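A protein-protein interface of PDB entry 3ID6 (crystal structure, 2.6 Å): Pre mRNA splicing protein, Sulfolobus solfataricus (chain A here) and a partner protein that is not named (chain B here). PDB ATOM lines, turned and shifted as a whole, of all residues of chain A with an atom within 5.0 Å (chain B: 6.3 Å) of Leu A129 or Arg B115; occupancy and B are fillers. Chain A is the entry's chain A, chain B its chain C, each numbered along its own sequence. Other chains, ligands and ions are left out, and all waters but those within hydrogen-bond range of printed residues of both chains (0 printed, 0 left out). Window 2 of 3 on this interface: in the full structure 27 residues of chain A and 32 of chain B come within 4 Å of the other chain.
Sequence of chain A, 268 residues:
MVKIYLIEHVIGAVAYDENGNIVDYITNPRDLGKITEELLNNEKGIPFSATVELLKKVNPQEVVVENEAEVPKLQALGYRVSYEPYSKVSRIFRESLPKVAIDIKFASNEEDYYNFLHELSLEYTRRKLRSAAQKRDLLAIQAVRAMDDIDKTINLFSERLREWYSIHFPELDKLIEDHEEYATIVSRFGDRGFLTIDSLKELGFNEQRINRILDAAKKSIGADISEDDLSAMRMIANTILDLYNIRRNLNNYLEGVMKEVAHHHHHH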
ATOM      1  N   THR A 125     -18.036  33.000   0.798  1.00  0.00           N
ATOM      2  CA  THR A 125     -18.217  32.107  -0.363  1.00  0.00           C
ATOM      3  C   THR A 125     -19.684  31.946  -0.820  1.00  0.00           C
ATOM      4  O   THR A 125     -19.941  31.827  -2.025  1.00  0.00           O
ATOM      5  CB  THR A 125     -17.478  30.738  -0.222  1.00  0.00           C
ATOM      6  OG1 THR A 125     -18.227  29.851   0.605  1.00  0.00           O
ATOM      7  CG2 THR A 125     -16.115  30.933   0.379  1.00  0.00           C
ATOM      8  N   ARG A 126     -20.631  31.962   0.126  1.00  0.00           N
ATOM      9  CA  ARG A 126     -22.067  32.002  -0.209  1.00  0.00           C
ATOM     10  C   ARG A 126     -22.416  33.234  -1.043  1.00  0.00           C
ATOM     11  O   ARG A 126     -23.164  33.137  -2.015  1.00  0.00           O
ATOM     12  CB  ARG A 126     -22.955  31.949   1.039  1.00  0.00           C
ATOM     13  CG  ARG A 126     -23.029  30.583   1.706  1.00  0.00           C
ATOM     14  CD  ARG A 126     -24.121  30.548   2.756  1.00  0.00           C
ATOM     15  NE  ARG A 126     -23.891  29.556   3.808  1.00  0.00           N
ATOM     16  CZ  ARG A 126     -23.554  29.850   5.069  1.00  0.00           C
ATOM     17  NH1 ARG A 126     -23.386  31.115   5.460  1.00  0.00           N
ATOM     18  NH2 ARG A 126     -23.378  28.874   5.951  1.00  0.00           N
ATOM     19  N   ARG A 127     -21.859  34.380  -0.660  1.00  0.00           N
ATOM     20  CA  ARG A 127     -22.018  35.631  -1.395  1.00  0.00           C
ATOM     21  C   ARG A 127     -21.495  35.485  -2.821  1.00  0.00           C
ATOM     22  O   ARG A 127     -22.219  35.734  -3.779  1.00  0.00           O
ATOM     23  CB  ARG A 127     -21.268  36.756  -0.681  1.00  0.00           C
ATOM     24  CG  ARG A 127     -21.672  38.168  -1.100  1.00  0.00           C
ATOM     25  CD  ARG A 127     -22.744  38.741  -0.177  1.00  0.00           C
ATOM     26  NE  ARG A 127     -22.565  38.297   1.209  1.00  0.00           N
ATOM     27  CZ  ARG A 127     -23.043  38.929   2.283  1.00  0.00           C
ATOM     28  NH1 ARG A 127     -23.733  40.060   2.158  1.00  0.00           N
ATOM     29  NH2 ARG A 127     -22.826  38.430   3.495  1.00  0.00           N
ATOM     30  N   LYS A 128     -20.237  35.061  -2.943  1.00  0.00           N
ATOM     31  CA  LYS A 128     -19.598  34.814  -4.237  1.00  0.00           C
ATOM     32  C   LYS A 128     -20.267  33.710  -5.063  1.00  0.00           C
ATOM     33  O   LYS A 128     -20.174  33.723  -6.288  1.00  0.00           O
ATOM     34  CB  LYS A 128     -18.107  34.509  -4.060  1.00  0.00           C
ATOM     35  CG  LYS A 128     -17.289  35.693  -3.550  1.00  0.00           C
ATOM     36  CD  LYS A 128     -15.772  35.437  -3.582  1.00  0.00           C
ATOM     37  CE  LYS A 128     -15.213  35.401  -5.028  1.00  0.00           C
ATOM     38  NZ  LYS A 128     -13.703  35.425  -5.081  1.00  0.00           N
ATOM     39  N   LEU A 129     -20.926  32.761  -4.398  1.00  0.00           N
ATOM     40  CA  LEU A 129     -21.718  31.749  -5.104  1.00  0.00           C
ATOM     41  C   LEU A 129     -22.908  32.376  -5.804  1.00  0.00           C
ATOM     42  O   LEU A 129     -23.083  32.212  -7.009  1.00  0.00           O
ATOM     43  CB  LEU A 129     -22.230  30.667  -4.152  1.00  0.00           C
ATOM     44  CG  LEU A 129     -21.553  29.301  -4.090  1.00  0.00           C
ATOM     45  CD1 LEU A 129     -22.672  28.278  -4.031  1.00  0.00           C
ATOM     46  CD2 LEU A 129     -20.658  29.022  -5.294  1.00  0.00           C
ATOM     47  N   ARG A 130     -23.722  33.099  -5.036  1.00  0.00           N
ATOM     48  CA  ARG A 130     -24.898  33.767  -5.580  1.00  0.00           C
ATOM     49  C   ARG A 130     -24.532  34.587  -6.787  1.00  0.00           C
ATOM     50  O   ARG A 130     -25.146  34.438  -7.840  1.00  0.00           O
ATOM     51  CB  ARG A 130     -25.574  34.657  -4.544  1.00  0.00           C
ATOM     52  CG  ARG A 130     -26.369  33.889  -3.512  1.00  0.00           C
ATOM     53  CD  ARG A 130     -27.302  34.810  -2.765  1.00  0.00           C
ATOM     54  NE  ARG A 130     -27.122  34.633  -1.327  1.00  0.00           N
ATOM     55  CZ  ARG A 130     -26.395  35.439  -0.557  1.00  0.00           C
ATOM     56  NH1 ARG A 130     -25.794  36.503  -1.086  1.00  0.00           N
ATOM     57  NH2 ARG A 130     -26.282  35.193   0.749  1.00  0.00           N
ATOM     58  N   SER A 131     -23.507  35.416  -6.643  1.00  0.00           N
ATOM     59  CA  SER A 131     -23.144  36.341  -7.693  1.00  0.00           C
ATOM     60  C   SER A 131     -22.527  35.639  -8.907  1.00  0.00           C
ATOM     61  O   SER A 131     -22.651  36.126 -10.016  1.00  0.00           O
ATOM     62  CB  SER A 131     -22.235  37.449  -7.147  1.00  0.00           C
ATOM     63  OG  SER A 131     -20.879  37.179  -7.443  1.00  0.00           O
ATOM     64  N   ALA A 132     -21.884  34.493  -8.699  1.00  0.00           N
ATOM     65  CA  ALA A 132     -21.373  33.687  -9.807  1.00  0.00           C
ATOM     66  C   ALA A 132     -22.528  32.999 -10.546  1.00  0.00           C
ATOM     67  O   ALA A 132     -22.478  32.827 -11.776  1.00  0.00           O
ATOM     68  CB  ALA A 132     -20.356  32.661  -9.324  1.00  0.00           C
ATOM     69  N   ALA A 133     -23.556  32.617  -9.789  1.00  0.00           N
ATOM     70  CA  ALA A 133     -24.750  32.019 -10.350  1.00  0.00           C
ATOM     71  C   ALA A 133     -25.583  33.060 -11.083  1.00  0.00           C
ATOM     72  O   ALA A 133     -26.152  32.776 -12.138  1.00  0.00           O
ATOM     73  CB  ALA A 133     -25.565  31.337  -9.273  1.00  0.00           C
ATOM     74  N   GLN A 134     -25.647  34.269 -10.534  1.00  0.00           N
ATOM     75  CA  GLN A 134     -26.368  35.365 -11.200  1.00  0.00           C
ATOM     76  C   GLN A 134     -25.723  35.756 -12.530  1.00  0.00           C
ATOM     77  O   GLN A 134     -26.411  35.878 -13.524  1.00  0.00           O
ATOM     78  CB  GLN A 134     -26.547  36.558 -10.262  1.00  0.00           C
ATOM     79  CG  GLN A 134     -27.438  36.206  -9.055  1.00  0.00           C
ATOM     80  CD  GLN A 134     -27.925  37.414  -8.261  1.00  0.00           C
ATOM     81  OE1 GLN A 134     -27.482  38.547  -8.484  1.00  0.00           O
ATOM     82  NE2 GLN A 134     -28.856  37.172  -7.333  1.00  0.00           N
ATOM     83  N   SER B 110     -14.681  26.175  -9.082  1.00  0.00           N
ATOM     84  CA  SER B 110     -15.943  25.760  -9.703  1.00  0.00           C
ATOM     85  C   SER B 110     -17.141  25.862  -8.764  1.00  0.00           C
ATOM     86  O   SER B 110     -17.193  25.156  -7.759  1.00  0.00           O
ATOM     87  CB  SER B 110     -15.828  24.325 -10.241  1.00  0.00           C
ATOM     88  OG  SER B 110     -17.100  23.723 -10.447  1.00  0.00           O
ATOM     89  N   PRO B 111     -18.115  26.732  -9.107  1.00  0.00           N
ATOM     90  CA  PRO B 111     -19.378  26.905  -8.377  1.00  0.00           C
ATOM     91  C   PRO B 111     -20.122  25.603  -8.045  1.00  0.00           C
ATOM     92  O   PRO B 111     -20.477  25.390  -6.882  1.00  0.00           O
ATOM     93  CB  PRO B 111     -20.207  27.775  -9.325  1.00  0.00           C
ATOM     94  CG  PRO B 111     -19.191  28.579 -10.058  1.00  0.00           C
ATOM     95  CD  PRO B 111     -18.024  27.654 -10.259  1.00  0.00           C
ATOM     96  N   ARG B 112     -20.355  24.744  -9.038  1.00  0.00           N
ATOM     97  CA  ARG B 112     -21.088  23.487  -8.818  1.00  0.00           C
ATOM     98  C   ARG B 112     -20.423  22.657  -7.722  1.00  0.00           C
ATOM     99  O   ARG B 112     -21.076  22.171  -6.799  1.00  0.00           O
ATOM    100  CB  ARG B 112     -21.177  22.678 -10.117  1.00  0.00           C
ATOM    101  CG  ARG B 112     -21.709  21.244  -9.960  1.00  0.00           C
ATOM    102  CD  ARG B 112     -21.721  20.482 -11.292  1.00  0.00           C
ATOM    103  NE  ARG B 112     -20.391  20.432 -11.912  1.00  0.00           N
ATOM    104  CZ  ARG B 112     -20.150  20.124 -13.190  1.00  0.00           C
ATOM    105  NH1 ARG B 112     -21.147  19.823 -14.027  1.00  0.00           N
ATOM    106  NH2 ARG B 112     -18.897  20.120 -13.635  1.00  0.00           N
ATOM    107  N   VAL B 113     -19.111  22.527  -7.841  1.00  0.00           N
ATOM    108  CA  VAL B 113     -18.294  21.734  -6.935  1.00  0.00           C
ATOM    109  C   VAL B 113     -18.231  22.364  -5.534  1.00  0.00           C
ATOM    110  O   VAL B 113     -18.447  21.679  -4.522  1.00  0.00           O
ATOM    111  CB  VAL B 113     -16.888  21.515  -7.569  1.00  0.00           C
ATOM    112  CG1 VAL B 113     -15.858  21.220  -6.541  1.00  0.00           C
ATOM    113  CG2 VAL B 113     -16.941  20.388  -8.608  1.00  0.00           C
ATOM    114  N   VAL B 114     -17.963  23.670  -5.489  1.00  0.00           N
ATOM    115  CA  VAL B 114     -17.928  24.442  -4.246  1.00  0.00           C
ATOM    116  C   VAL B 114     -19.201  24.303  -3.417  1.00  0.00           C
ATOM    117  O   VAL B 114     -19.130  24.219  -2.193  1.00  0.00           O
ATOM    118  CB  VAL B 114     -17.639  25.940  -4.522  1.00  0.00           C
ATOM    119  CG1 VAL B 114     -18.203  26.840  -3.420  1.00  0.00           C
ATOM    120  CG2 VAL B 114     -16.163  26.155  -4.663  1.00  0.00           C
ATOM    121  N   ARG B 115     -20.351  24.276  -4.086  1.00  0.00           N
ATOM    122  CA  ARG B 115     -21.643  24.172  -3.406  1.00  0.00           C
ATOM    123  C   ARG B 115     -21.687  22.962  -2.475  1.00  0.00           C
ATOM    124  O   ARG B 115     -22.311  23.014  -1.418  1.00  0.00           O
ATOM    125  CB  ARG B 115     -22.792  24.116  -4.421  1.00  0.00           C
ATOM    126  CG  ARG B 115     -24.129  24.582  -3.866  1.00  0.00           C
ATOM    127  CD  ARG B 115     -25.143  24.875  -4.977  1.00  0.00           C
ATOM    128  NE  ARG B 115     -25.971  23.715  -5.303  1.00  0.00           N
ATOM    129  CZ  ARG B 115     -25.737  22.862  -6.299  1.00  0.00           C
ATOM    130  NH1 ARG B 115     -26.566  21.844  -6.500  1.00  0.00           N
ATOM    131  NH2 ARG B 115     -24.688  23.019  -7.099  1.00  0.00           N
ATOM    132  N   GLU B 116     -21.010  21.886  -2.876  1.00  0.00           N
ATOM    133  CA  GLU B 116     -20.932  20.662  -2.073  1.00  0.00           C
ATOM    134  C   GLU B 116     -19.838  20.743  -1.014  1.00  0.00           C
ATOM    135  O   GLU B 116     -19.957  20.126   0.040  1.00  0.00           O
ATOM    136  CB  GLU B 116     -20.751  19.421  -2.961  1.00  0.00           C
ATOM    137  CG  GLU B 116     -22.013  19.038  -3.754  1.00  0.00           C
ATOM    138  CD  GLU B 116     -21.785  17.920  -4.776  1.00  0.00           C
ATOM    139  OE1 GLU B 116     -20.643  17.772  -5.273  1.00  0.00           O
ATOM    140  OE2 GLU B 116     -22.759  17.191  -5.098  1.00  0.00           O
ATOM    141  N   LEU B 117     -18.787  21.514  -1.293  1.00  0.00           N
ATOM    142  CA  LEU B 117     -17.724  21.793  -0.321  1.00  0.00           C
ATOM    143  C   LEU B 117     -18.234  22.587   0.881  1.00  0.00           C
ATOM    144  O   LEU B 117     -17.635  22.547   1.953  1.00  0.00           O
ATOM    145  CB  LEU B 117     -16.561  22.538  -0.991  1.00  0.00           C
ATOM    146  CG  LEU B 117     -15.362  23.029  -0.163  1.00  0.00           C
ATOM    147  CD1 LEU B 117     -14.574  21.869   0.410  1.00  0.00           C
ATOM    148  CD2 LEU B 117     -14.452  23.932  -0.979  1.00  0.00           C
ATOM    149  N   LEU B 118     -19.328  23.321   0.701  1.00  0.00           N
ATOM    150  CA  LEU B 118     -19.955  24.039   1.804  1.00  0.00           C
ATOM    151  C   LEU B 118     -20.545  23.073   2.832  1.00  0.00           C
ATOM    152  O   LEU B 118     -20.363  23.269   4.037  1.00  0.00           O
ATOM    153  CB  LEU B 118     -21.038  25.003   1.307  1.00  0.00           C
ATOM    154  CG  LEU B 118     -20.622  26.357   0.722  1.00  0.00           C
ATOM    155  CD1 LEU B 118     -21.845  27.073   0.175  1.00  0.00           C
ATOM    156  CD2 LEU B 118     -19.893  27.248   1.736  1.00  0.00           C
ATOM    157  N   LEU B 119     -21.228  22.033   2.354  1.00  0.00           N
ATOM    158  CA  LEU B 119     -21.846  21.037   3.230  1.00  0.00           C
ATOM    159  C   LEU B 119     -20.826  20.378   4.156  1.00  0.00           C
ATOM    160  O   LEU B 119     -21.084  20.186   5.342  1.00  0.00           O
ATOM    161  CB  LEU B 119     -22.605  19.982   2.419  1.00  0.00           C
ATOM    162  CG  LEU B 119     -23.883  20.442   1.701  1.00  0.00           C
ATOM    163  CD1 LEU B 119     -24.520  19.305   0.881  1.00  0.00           C
ATOM    164  CD2 LEU B 119     -24.906  21.039   2.681  1.00  0.00           C
ATOM    165  N   LEU B 131     -14.356  30.131  -2.579  1.00  0.00           N
ATOM    166  CA  LEU B 131     -14.484  30.235  -4.023  1.00  0.00           C
ATOM    167  C   LEU B 131     -13.495  31.289  -4.503  1.00  0.00           C
ATOM    168  O   LEU B 131     -13.672  32.489  -4.240  1.00  0.00           O
ATOM    169  CB  LEU B 131     -15.909  30.587  -4.472  1.00  0.00           C
ATOM    170  CG  LEU B 131     -16.077  30.720  -5.994  1.00  0.00           C
ATOM    171  CD1 LEU B 131     -16.033  29.360  -6.665  1.00  0.00           C
ATOM    172  CD2 LEU B 131     -17.361  31.439  -6.358  1.00  0.00           C
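The backbone carbonyl oxygen (O) of Leu B131 lies within hydrogen-bond range of the side-chain amino group (NZ) of Lys A128 (3.1 Å).
Among the printed residues, merely in contact across the chains: Thr A125 with Leu B118, Thr A125 with Leu B131, Leu A129 with Val B114, Leu A129 with Pro B111 and Leu A129 with Arg B115.
Leu A129 touches just these residues of chain B: Pro B111 (3.95 Å), Val B114 (3.8 Å) and Arg B115 (3.98 Å).
Of chain A, only Leu A129 comes within 4 Å of Arg B115.
Printed residues of chain A within 4 Å of Leu B131: Thr A125 and Lys A128.
Printed residues of chain A within 4 Å of Pro B111: Leu A129.
The nearest residue of chain B that does not touch Leu A129 is Leu B131 (4.2 Å).
Of the 10 printed residues of chain A, 3 touch a printed residue of chain B.
Printed residues of chain A that touch a printed residue of chain B: Thr A125, Lys A128 and Leu A129.
Hydrophobic or aromatic side chains of chain A within 4 Å of the printed part of chain B: Leu A129.
Among the printed residues, no Asp or Glu carboxylate lies within 4 Å of a Lys or Arg side-chain nitrogen of the other chain.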
